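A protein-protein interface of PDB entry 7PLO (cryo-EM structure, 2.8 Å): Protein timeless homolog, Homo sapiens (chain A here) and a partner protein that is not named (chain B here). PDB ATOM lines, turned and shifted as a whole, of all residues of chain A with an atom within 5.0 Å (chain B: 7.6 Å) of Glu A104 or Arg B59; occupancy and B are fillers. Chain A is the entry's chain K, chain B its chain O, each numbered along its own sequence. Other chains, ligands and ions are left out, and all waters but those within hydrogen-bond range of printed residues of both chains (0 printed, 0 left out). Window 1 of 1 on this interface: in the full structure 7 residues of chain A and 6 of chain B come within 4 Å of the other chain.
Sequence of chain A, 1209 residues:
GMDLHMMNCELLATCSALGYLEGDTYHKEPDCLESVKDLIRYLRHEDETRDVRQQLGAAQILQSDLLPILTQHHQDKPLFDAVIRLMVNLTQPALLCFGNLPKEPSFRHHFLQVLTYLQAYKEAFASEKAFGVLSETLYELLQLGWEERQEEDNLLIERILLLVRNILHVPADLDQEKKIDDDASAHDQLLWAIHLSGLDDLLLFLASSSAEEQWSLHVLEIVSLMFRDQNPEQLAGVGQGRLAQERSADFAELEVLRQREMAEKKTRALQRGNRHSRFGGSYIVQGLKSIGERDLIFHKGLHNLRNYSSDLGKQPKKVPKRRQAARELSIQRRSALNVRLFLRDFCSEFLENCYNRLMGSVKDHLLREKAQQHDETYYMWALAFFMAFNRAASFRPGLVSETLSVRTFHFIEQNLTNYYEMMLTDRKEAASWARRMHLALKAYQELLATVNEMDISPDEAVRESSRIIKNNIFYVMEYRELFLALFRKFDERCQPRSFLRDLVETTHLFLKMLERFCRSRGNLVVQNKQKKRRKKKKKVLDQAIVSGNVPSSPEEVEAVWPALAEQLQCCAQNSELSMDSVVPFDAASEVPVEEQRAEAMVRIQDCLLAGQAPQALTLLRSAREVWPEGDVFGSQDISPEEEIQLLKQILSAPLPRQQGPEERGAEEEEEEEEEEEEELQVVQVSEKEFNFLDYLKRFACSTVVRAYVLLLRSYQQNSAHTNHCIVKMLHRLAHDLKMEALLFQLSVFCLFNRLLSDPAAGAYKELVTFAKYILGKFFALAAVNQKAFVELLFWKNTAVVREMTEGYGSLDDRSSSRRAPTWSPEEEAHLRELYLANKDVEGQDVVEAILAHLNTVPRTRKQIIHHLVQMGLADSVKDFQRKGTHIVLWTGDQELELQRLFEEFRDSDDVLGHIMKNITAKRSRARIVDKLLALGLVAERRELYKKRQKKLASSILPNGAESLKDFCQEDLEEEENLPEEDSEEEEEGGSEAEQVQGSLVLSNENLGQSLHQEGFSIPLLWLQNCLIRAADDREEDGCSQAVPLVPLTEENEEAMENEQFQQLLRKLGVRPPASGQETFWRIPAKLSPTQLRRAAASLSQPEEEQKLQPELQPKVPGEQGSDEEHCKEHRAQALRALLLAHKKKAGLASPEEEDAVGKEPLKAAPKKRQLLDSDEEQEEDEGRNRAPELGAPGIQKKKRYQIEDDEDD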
ATOM      1  N   THR A  49     -17.201 -18.795  15.973  1.00  0.00           N
ATOM      2  CA  THR A  49     -17.342 -17.464  16.554  1.00  0.00           C
ATOM      3  C   THR A  49     -18.768 -16.925  16.475  1.00  0.00           C
ATOM      4  O   THR A  49     -19.035 -15.868  17.057  1.00  0.00           O
ATOM      5  CB  THR A  49     -16.398 -16.478  15.858  1.00  0.00           C
ATOM      6  OG1 THR A  49     -16.738 -16.379  14.469  1.00  0.00           O
ATOM      7  CG2 THR A  49     -14.942 -16.920  15.994  1.00  0.00           C
ATOM      8  N   PRO A 102     -16.081 -18.631  27.688  1.00  0.00           N
ATOM      9  CA  PRO A 102     -14.709 -18.780  27.183  1.00  0.00           C
ATOM     10  C   PRO A 102     -13.667 -18.239  28.150  1.00  0.00           C
ATOM     11  O   PRO A 102     -13.904 -17.280  28.888  1.00  0.00           O
ATOM     12  CB  PRO A 102     -14.721 -17.976  25.882  1.00  0.00           C
ATOM     13  CG  PRO A 102     -16.137 -17.935  25.485  1.00  0.00           C
ATOM     14  CD  PRO A 102     -16.897 -17.847  26.740  1.00  0.00           C
ATOM     15  N   LYS A 103     -12.494 -18.873  28.129  1.00  0.00           N
ATOM     16  CA  LYS A 103     -11.396 -18.527  29.020  1.00  0.00           C
ATOM     17  C   LYS A 103     -10.416 -17.518  28.431  1.00  0.00           C
ATOM     18  O   LYS A 103      -9.522 -17.075  29.161  1.00  0.00           O
ATOM     19  CB  LYS A 103     -10.622 -19.791  29.415  1.00  0.00           C
ATOM     20  CG  LYS A 103     -11.396 -20.744  30.317  1.00  0.00           C
ATOM     21  CD  LYS A 103     -10.510 -21.855  30.875  1.00  0.00           C
ATOM     22  CE  LYS A 103     -10.044 -22.820  29.792  1.00  0.00           C
ATOM     23  NZ  LYS A 103      -9.338 -24.001  30.361  1.00  0.00           N
ATOM     24  N   GLU A 104     -10.556 -17.141  27.157  1.00  0.00           N
ATOM     25  CA  GLU A 104      -9.634 -16.254  26.461  1.00  0.00           C
ATOM     26  C   GLU A 104     -10.377 -15.058  25.867  1.00  0.00           C
ATOM     27  O   GLU A 104     -11.591 -15.130  25.638  1.00  0.00           O
ATOM     28  CB  GLU A 104      -8.873 -17.008  25.358  1.00  0.00           C
ATOM     29  CG  GLU A 104      -9.734 -17.549  24.206  1.00  0.00           C
ATOM     30  CD  GLU A 104      -9.876 -16.597  23.018  1.00  0.00           C
ATOM     31  OE1 GLU A 104      -9.053 -15.671  22.853  1.00  0.00           O
ATOM     32  OE2 GLU A 104     -10.831 -16.785  22.236  1.00  0.00           O
ATOM     33  N   PRO A 105      -9.683 -13.931  25.617  1.00  0.00           N
ATOM     34  CA  PRO A 105     -10.409 -12.680  25.311  1.00  0.00           C
ATOM     35  C   PRO A 105     -11.256 -12.688  24.046  1.00  0.00           C
ATOM     36  O   PRO A 105     -12.324 -12.068  24.043  1.00  0.00           O
ATOM     37  CB  PRO A 105      -9.281 -11.642  25.206  1.00  0.00           C
ATOM     38  CG  PRO A 105      -8.149 -12.223  25.939  1.00  0.00           C
ATOM     39  CD  PRO A 105      -8.229 -13.685  25.684  1.00  0.00           C
ATOM     40  N   SER A 106     -10.817 -13.337  22.967  1.00  0.00           N
ATOM     41  CA  SER A 106     -11.521 -13.191  21.693  1.00  0.00           C
ATOM     42  C   SER A 106     -12.892 -13.864  21.728  1.00  0.00           C
ATOM     43  O   SER A 106     -13.915 -13.246  21.390  1.00  0.00           O
ATOM     44  CB  SER A 106     -10.666 -13.762  20.563  1.00  0.00           C
ATOM     45  OG  SER A 106      -9.413 -13.104  20.498  1.00  0.00           O
ATOM     46  N   PHE A 107     -12.935 -15.132  22.147  1.00  0.00           N
ATOM     47  CA  PHE A 107     -14.220 -15.810  22.264  1.00  0.00           C
ATOM     48  C   PHE A 107     -15.092 -15.157  23.326  1.00  0.00           C
ATOM     49  O   PHE A 107     -16.318 -15.174  23.204  1.00  0.00           O
ATOM     50  CB  PHE A 107     -14.036 -17.298  22.618  1.00  0.00           C
ATOM     51  CG  PHE A 107     -13.982 -18.271  21.441  1.00  0.00           C
ATOM     52  CD1 PHE A 107     -14.774 -18.136  20.303  1.00  0.00           C
ATOM     53  CD2 PHE A 107     -13.168 -19.385  21.536  1.00  0.00           C
ATOM     54  CE1 PHE A 107     -14.701 -19.054  19.275  1.00  0.00           C
ATOM     55  CE2 PHE A 107     -13.096 -20.307  20.511  1.00  0.00           C
ATOM     56  CZ  PHE A 107     -13.866 -20.141  19.382  1.00  0.00           C
ATOM     57  N   ARG A 108     -14.493 -14.586  24.373  1.00  0.00           N
ATOM     58  CA  ARG A 108     -15.302 -13.909  25.384  1.00  0.00           C
ATOM     59  C   ARG A 108     -15.914 -12.630  24.826  1.00  0.00           C
ATOM     60  O   ARG A 108     -17.048 -12.281  25.168  1.00  0.00           O
ATOM     61  CB  ARG A 108     -14.464 -13.618  26.634  1.00  0.00           C
ATOM     62  CG  ARG A 108     -15.239 -13.028  27.834  1.00  0.00           C
ATOM     63  CD  ARG A 108     -16.212 -14.013  28.484  1.00  0.00           C
ATOM     64  NE  ARG A 108     -15.517 -15.001  29.309  1.00  0.00           N
ATOM     65  CZ  ARG A 108     -15.455 -15.025  30.639  1.00  0.00           C
ATOM     66  NH1 ARG A 108     -16.084 -14.134  31.394  1.00  0.00           N
ATOM     67  NH2 ARG A 108     -14.746 -15.979  31.232  1.00  0.00           N
ATOM     68  N   HIS A 110     -16.771 -12.285  21.684  1.00  0.00           N
ATOM     69  CA  HIS A 110     -17.875 -12.772  20.858  1.00  0.00           C
ATOM     70  C   HIS A 110     -19.067 -13.201  21.715  1.00  0.00           C
ATOM     71  O   HIS A 110     -20.228 -12.954  21.354  1.00  0.00           O
ATOM     72  CB  HIS A 110     -17.386 -13.918  19.976  1.00  0.00           C
ATOM     73  CG  HIS A 110     -16.283 -13.524  19.044  1.00  0.00           C
ATOM     74  ND1 HIS A 110     -16.262 -12.312  18.387  1.00  0.00           N
ATOM     75  CD2 HIS A 110     -15.154 -14.173  18.669  1.00  0.00           C
ATOM     76  CE1 HIS A 110     -15.175 -12.236  17.640  1.00  0.00           C
ATOM     77  NE2 HIS A 110     -14.485 -13.351  17.795  1.00  0.00           N
ATOM     78  N   ARG B  44     -11.555 -25.696  12.859  1.00  0.00           N
ATOM     79  CA  ARG B  44     -11.062 -24.634  11.993  1.00  0.00           C
ATOM     80  C   ARG B  44      -9.843 -23.977  12.631  1.00  0.00           C
ATOM     81  O   ARG B  44      -9.698 -23.953  13.857  1.00  0.00           O
ATOM     82  CB  ARG B  44     -12.152 -23.584  11.722  1.00  0.00           C
ATOM     83  CG  ARG B  44     -13.483 -24.131  11.161  1.00  0.00           C
ATOM     84  CD  ARG B  44     -13.406 -24.537   9.685  1.00  0.00           C
ATOM     85  NE  ARG B  44     -12.652 -25.767   9.470  1.00  0.00           N
ATOM     86  CZ  ARG B  44     -12.495 -26.379   8.302  1.00  0.00           C
ATOM     87  NH1 ARG B  44     -13.055 -25.920   7.191  1.00  0.00           N
ATOM     88  NH2 ARG B  44     -11.756 -27.484   8.244  1.00  0.00           N
ATOM     89  N   ALA B  45      -8.968 -23.442  11.783  1.00  0.00           N
ATOM     90  CA  ALA B  45      -7.630 -23.058  12.216  1.00  0.00           C
ATOM     91  C   ALA B  45      -7.641 -21.798  13.077  1.00  0.00           C
ATOM     92  O   ALA B  45      -8.373 -20.842  12.804  1.00  0.00           O
ATOM     93  CB  ALA B  45      -6.729 -22.844  11.001  1.00  0.00           C
ATOM     94  N   PHE B  46      -6.804 -21.806  14.117  1.00  0.00           N
ATOM     95  CA  PHE B  46      -6.552 -20.668  14.991  1.00  0.00           C
ATOM     96  C   PHE B  46      -5.051 -20.443  15.105  1.00  0.00           C
ATOM     97  O   PHE B  46      -4.250 -21.371  14.920  1.00  0.00           O
ATOM     98  CB  PHE B  46      -7.086 -20.880  16.420  1.00  0.00           C
ATOM     99  CG  PHE B  46      -8.551 -21.206  16.509  1.00  0.00           C
ATOM    100  CD1 PHE B  46      -9.472 -20.658  15.632  1.00  0.00           C
ATOM    101  CD2 PHE B  46      -9.008 -22.052  17.506  1.00  0.00           C
ATOM    102  CE1 PHE B  46     -10.816 -20.962  15.737  1.00  0.00           C
ATOM    103  CE2 PHE B  46     -10.348 -22.359  17.617  1.00  0.00           C
ATOM    104  CZ  PHE B  46     -11.255 -21.813  16.732  1.00  0.00           C
ATOM    105  N   LEU B  47      -4.681 -19.207  15.459  1.00  0.00           N
ATOM    106  CA  LEU B  47      -3.339 -18.891  15.947  1.00  0.00           C
ATOM    107  C   LEU B  47      -3.441 -18.516  17.419  1.00  0.00           C
ATOM    108  O   LEU B  47      -4.108 -17.537  17.758  1.00  0.00           O
ATOM    109  CB  LEU B  47      -2.703 -17.749  15.150  1.00  0.00           C
ATOM    110  CG  LEU B  47      -1.431 -17.100  15.726  1.00  0.00           C
ATOM    111  CD1 LEU B  47      -0.339 -18.131  15.997  1.00  0.00           C
ATOM    112  CD2 LEU B  47      -0.907 -16.020  14.801  1.00  0.00           C
ATOM    113  N   LEU B  48      -2.758 -19.271  18.278  1.00  0.00           N
ATOM    114  CA  LEU B  48      -2.677 -18.983  19.707  1.00  0.00           C
ATOM    115  C   LEU B  48      -1.340 -18.316  19.997  1.00  0.00           C
ATOM    116  O   LEU B  48      -0.287 -18.871  19.665  1.00  0.00           O
ATOM    117  CB  LEU B  48      -2.813 -20.263  20.533  1.00  0.00           C
ATOM    118  CG  LEU B  48      -4.207 -20.803  20.867  1.00  0.00           C
ATOM    119  CD1 LEU B  48      -4.895 -19.924  21.900  1.00  0.00           C
ATOM    120  CD2 LEU B  48      -5.071 -20.956  19.620  1.00  0.00           C
ATOM    121  N   ILE B  49      -1.383 -17.138  20.619  1.00  0.00           N
ATOM    122  CA  ILE B  49      -0.192 -16.421  21.070  1.00  0.00           C
ATOM    123  C   ILE B  49      -0.231 -16.414  22.591  1.00  0.00           C
ATOM    124  O   ILE B  49      -1.173 -15.874  23.185  1.00  0.00           O
ATOM    125  CB  ILE B  49      -0.129 -14.989  20.503  1.00  0.00           C
ATOM    126  CG1 ILE B  49      -0.289 -15.031  18.971  1.00  0.00           C
ATOM    127  CG2 ILE B  49       1.193 -14.281  20.929  1.00  0.00           C
ATOM    128  CD1 ILE B  49      -0.055 -13.712  18.233  1.00  0.00           C
ATOM    129  N   SER B  50       0.799 -16.998  23.215  1.00  0.00           N
ATOM    130  CA  SER B  50       0.912 -17.067  24.668  1.00  0.00           C
ATOM    131  C   SER B  50       2.221 -16.433  25.113  1.00  0.00           C
ATOM    132  O   SER B  50       3.268 -16.659  24.499  1.00  0.00           O
ATOM    133  CB  SER B  50       0.845 -18.514  25.163  1.00  0.00           C
ATOM    134  OG  SER B  50      -0.422 -19.090  24.900  1.00  0.00           O
ATOM    135  N   ASP B  54       0.134 -14.475  29.893  1.00  0.00           N
ATOM    136  CA  ASP B  54      -1.016 -15.344  29.636  1.00  0.00           C
ATOM    137  C   ASP B  54      -0.518 -16.694  29.124  1.00  0.00           C
ATOM    138  O   ASP B  54      -0.167 -16.826  27.949  1.00  0.00           O
ATOM    139  CB  ASP B  54      -1.972 -14.691  28.646  1.00  0.00           C
ATOM    140  CG  ASP B  54      -1.252 -14.066  27.465  1.00  0.00           C
ATOM    141  OD1 ASP B  54      -0.010 -14.176  27.397  1.00  0.00           O
ATOM    142  OD2 ASP B  54      -1.929 -13.462  26.606  1.00  0.00           O
ATOM    143  N   ARG B  56      -2.776 -19.063  29.136  1.00  0.00           N
ATOM    144  CA  ARG B  56      -3.984 -19.195  28.323  1.00  0.00           C
ATOM    145  C   ARG B  56      -3.976 -18.045  27.327  1.00  0.00           C
ATOM    146  O   ARG B  56      -4.519 -16.967  27.576  1.00  0.00           O
ATOM    147  CB  ARG B  56      -5.234 -19.183  29.195  1.00  0.00           C
ATOM    148  CG  ARG B  56      -5.275 -20.291  30.239  1.00  0.00           C
ATOM    149  CD  ARG B  56      -6.689 -20.520  30.762  1.00  0.00           C
ATOM    150  NE  ARG B  56      -7.255 -19.309  31.362  1.00  0.00           N
ATOM    151  CZ  ARG B  56      -7.713 -19.168  32.604  1.00  0.00           C
ATOM    152  NH1 ARG B  56      -7.745 -20.173  33.470  1.00  0.00           N
ATOM    153  NH2 ARG B  56      -8.166 -17.979  32.991  1.00  0.00           N
ATOM    154  N   GLY B  57      -3.350 -18.282  26.178  1.00  0.00           N
ATOM    155  CA  GLY B  57      -3.057 -17.213  25.249  1.00  0.00           C
ATOM    156  C   GLY B  57      -4.262 -16.728  24.469  1.00  0.00           C
ATOM    157  O   GLY B  57      -5.363 -17.275  24.541  1.00  0.00           O
ATOM    158  N   THR B  58      -4.023 -15.668  23.703  1.00  0.00           N
ATOM    159  CA  THR B  58      -5.044 -15.064  22.858  1.00  0.00           C
ATOM    160  C   THR B  58      -5.117 -15.793  21.523  1.00  0.00           C
ATOM    161  O   THR B  58      -4.085 -16.064  20.899  1.00  0.00           O
ATOM    162  CB  THR B  58      -4.746 -13.582  22.619  1.00  0.00           C
ATOM    163  OG1 THR B  58      -3.330 -13.380  22.535  1.00  0.00           O
ATOM    164  CG2 THR B  58      -5.320 -12.725  23.735  1.00  0.00           C
ATOM    165  N   ARG B  59      -6.336 -16.116  21.099  1.00  0.00           N
ATOM    166  CA  ARG B  59      -6.563 -16.639  19.763  1.00  0.00           C
ATOM    167  C   ARG B  59      -6.635 -15.506  18.748  1.00  0.00           C
ATOM    168  O   ARG B  59      -6.898 -14.347  19.083  1.00  0.00           O
ATOM    169  CB  ARG B  59      -7.864 -17.426  19.690  1.00  0.00           C
ATOM    170  CG  ARG B  59      -7.979 -18.609  20.638  1.00  0.00           C
ATOM    171  CD  ARG B  59      -9.266 -19.408  20.400  1.00  0.00           C
ATOM    172  NE  ARG B  59     -10.433 -18.541  20.231  1.00  0.00           N
ATOM    173  CZ  ARG B  59     -10.962 -18.146  19.076  1.00  0.00           C
ATOM    174  NH1 ARG B  59     -10.516 -18.586  17.909  1.00  0.00           N
ATOM    175  NH2 ARG B  59     -11.962 -17.270  19.091  1.00  0.00           N
ATOM    176  N   TYR B  60      -6.398 -15.860  17.489  1.00  0.00           N
ATOM    177  CA  TYR B  60      -6.629 -14.969  16.361  1.00  0.00           C
ATOM    178  C   TYR B  60      -7.114 -15.805  15.188  1.00  0.00           C
ATOM    179  O   TYR B  60      -6.524 -16.850  14.876  1.00  0.00           O
ATOM    180  CB  TYR B  60      -5.365 -14.187  15.979  1.00  0.00           C
ATOM    181  CG  TYR B  60      -4.864 -13.278  17.078  1.00  0.00           C
ATOM    182  CD1 TYR B  60      -5.428 -12.026  17.285  1.00  0.00           C
ATOM    183  CD2 TYR B  60      -3.842 -13.682  17.922  1.00  0.00           C
ATOM    184  CE1 TYR B  60      -4.976 -11.199  18.296  1.00  0.00           C
ATOM    185  CE2 TYR B  60      -3.386 -12.864  18.934  1.00  0.00           C
ATOM    186  CZ  TYR B  60      -3.954 -11.623  19.117  1.00  0.00           C
ATOM    187  OH  TYR B  60      -3.496 -10.809  20.126  1.00  0.00           O
ATOM    188  N   GLU B  61      -8.201 -15.347  14.567  1.00  0.00           N
ATOM    189  CA  GLU B  61      -8.739 -16.017  13.392  1.00  0.00           C
ATOM    190  C   GLU B  61      -7.859 -15.712  12.189  1.00  0.00           C
ATOM    191  O   GLU B  61      -7.427 -14.573  11.991  1.00  0.00           O
ATOM    192  CB  GLU B  61     -10.178 -15.570  13.097  1.00  0.00           C
ATOM    193  CG  GLU B  61     -11.088 -15.353  14.305  1.00  0.00           C
ATOM    194  CD  GLU B  61     -11.108 -16.526  15.261  1.00  0.00           C
ATOM    195  OE1 GLU B  61     -10.809 -17.660  14.830  1.00  0.00           O
ATOM    196  OE2 GLU B  61     -11.422 -16.314  16.451  1.00  0.00           O
ATOM    197  N   LEU B  62      -7.586 -16.748  11.390  1.00  0.00           N
ATOM    198  CA  LEU B  62      -6.799 -16.594  10.173  1.00  0.00           C
ATOM    199  C   LEU B  62      -7.342 -17.452   9.033  1.00  0.00           C
ATOM    200  O   LEU B  62      -6.600 -17.752   8.093  1.00  0.00           O
ATOM    201  CB  LEU B  62      -5.317 -16.924  10.453  1.00  0.00           C
ATOM    202  CG  LEU B  62      -4.957 -18.174  11.272  1.00  0.00           C
ATOM    203  CD1 LEU B  62      -5.351 -19.481  10.591  1.00  0.00           C
ATOM    204  CD2 LEU B  62      -3.467 -18.166  11.559  1.00  0.00           C
ATOM    205  N   GLU B  85      -3.375  -8.003   9.720  1.00  0.00           N
ATOM    206  CA  GLU B  85      -4.679  -8.644   9.645  1.00  0.00           C
ATOM    207  C   GLU B  85      -5.739  -7.575   9.845  1.00  0.00           C
ATOM    208  O   GLU B  85      -5.419  -6.424  10.167  1.00  0.00           O
ATOM    209  CB  GLU B  85      -4.838  -9.736  10.711  1.00  0.00           C
ATOM    210  CG  GLU B  85      -3.823 -10.858  10.658  1.00  0.00           C
ATOM    211  CD  GLU B  85      -4.008 -11.845  11.792  1.00  0.00           C
ATOM    212  OE1 GLU B  85      -5.068 -11.802  12.451  1.00  0.00           O
ATOM    213  OE2 GLU B  85      -3.091 -12.658  12.031  1.00  0.00           O
ATOM    214  N   VAL B  88      -5.342  -6.191  13.518  1.00  0.00           N
ATOM    215  CA  VAL B  88      -4.079  -6.205  14.256  1.00  0.00           C
ATOM    216  C   VAL B  88      -2.888  -6.449  13.335  1.00  0.00           C
ATOM    217  O   VAL B  88      -3.045  -6.848  12.177  1.00  0.00           O
ATOM    218  CB  VAL B  88      -4.102  -7.250  15.392  1.00  0.00           C
ATOM    219  CG1 VAL B  88      -5.152  -6.884  16.433  1.00  0.00           C
ATOM    220  CG2 VAL B  88      -4.328  -8.676  14.862  1.00  0.00           C
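Of the 17 printed residues of chain B, 5 touch a printed residue of chain A.
Printed residues of chain A that touch a printed residue of chain B: Thr A49, Lys A103, Glu A104, Pro A105, Ser A106 and Phe A107.
Hydrophobic or aromatic side chains of chain A that line the printed part of chain B: Pro A105 and Phe A107.
Among the printed residues, 7 pairs touch across the chains.
Of the printed residues of chain B, Thr A49 touches Glu B61.
Of the printed residues of chain B, Pro A105 touches Thr B58 (3.6 Å).
Of the printed residues of chain B, Ser A106 touches Arg B59 (3.1 Å).
Ala B45 touches none of the printed residues of chain A.
Of the printed residues of chain A, Arg B56 touches Lys A103.
Printed residues of chain A within 4 Å of Gly B57: Glu A104.
Printed residues of chain A within 4 Å of Arg B59: Glu A104, Ser A106 and Phe A107.
Tyr B60 touches none of the printed residues of chain A.
The nearest residue of chain B that does not touch Glu A104 is Thr B58 (4.1 Å).
The nearest residue of chain A that does not touch Arg B59 is Thr A49 (4.3 Å).
The guanidinium group of Arg B59 is in salt-bridge range of the side-chain carboxylate of Glu A104, 2.7 Å away.
The backbone carbonyl oxygen of Arg B59 lies within hydrogen-bond range of the side-chain hydroxyl of Ser A106 (3.1 Å).
NH1 of Arg B59 lies within salt-bridge range of OE2 of Glu B61.
The side-chain hydroxyl (OG) of Ser B50 sits close to the backbone NH (N) of Gly B57 (3.3 Å).
OE2 of Glu A104 is in hydrogen-bond range of N of Phe A107 (2.7 Å).
The side-chain carboxylate (OE1) of Glu A104 lies within hydrogen-bond range of the backbone NH (N) of Ser A106, 2.9 Å away.
N of Thr B58 lies within hydrogen-bond range of O of Ile B49, 2.9 Å away.
Thr A49 touches Glu B61 (CG2 to OE2, 3.6 Å).
O of Lys A103 touches NE of Arg B56, 3.9 Å away.
O of Gly B57 touches CB of Glu A104, 3.6 Å away.
Thr B58 touches Pro A105 (CG2 to CG, 3.6 Å).
Phe A107 touches Arg B59.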
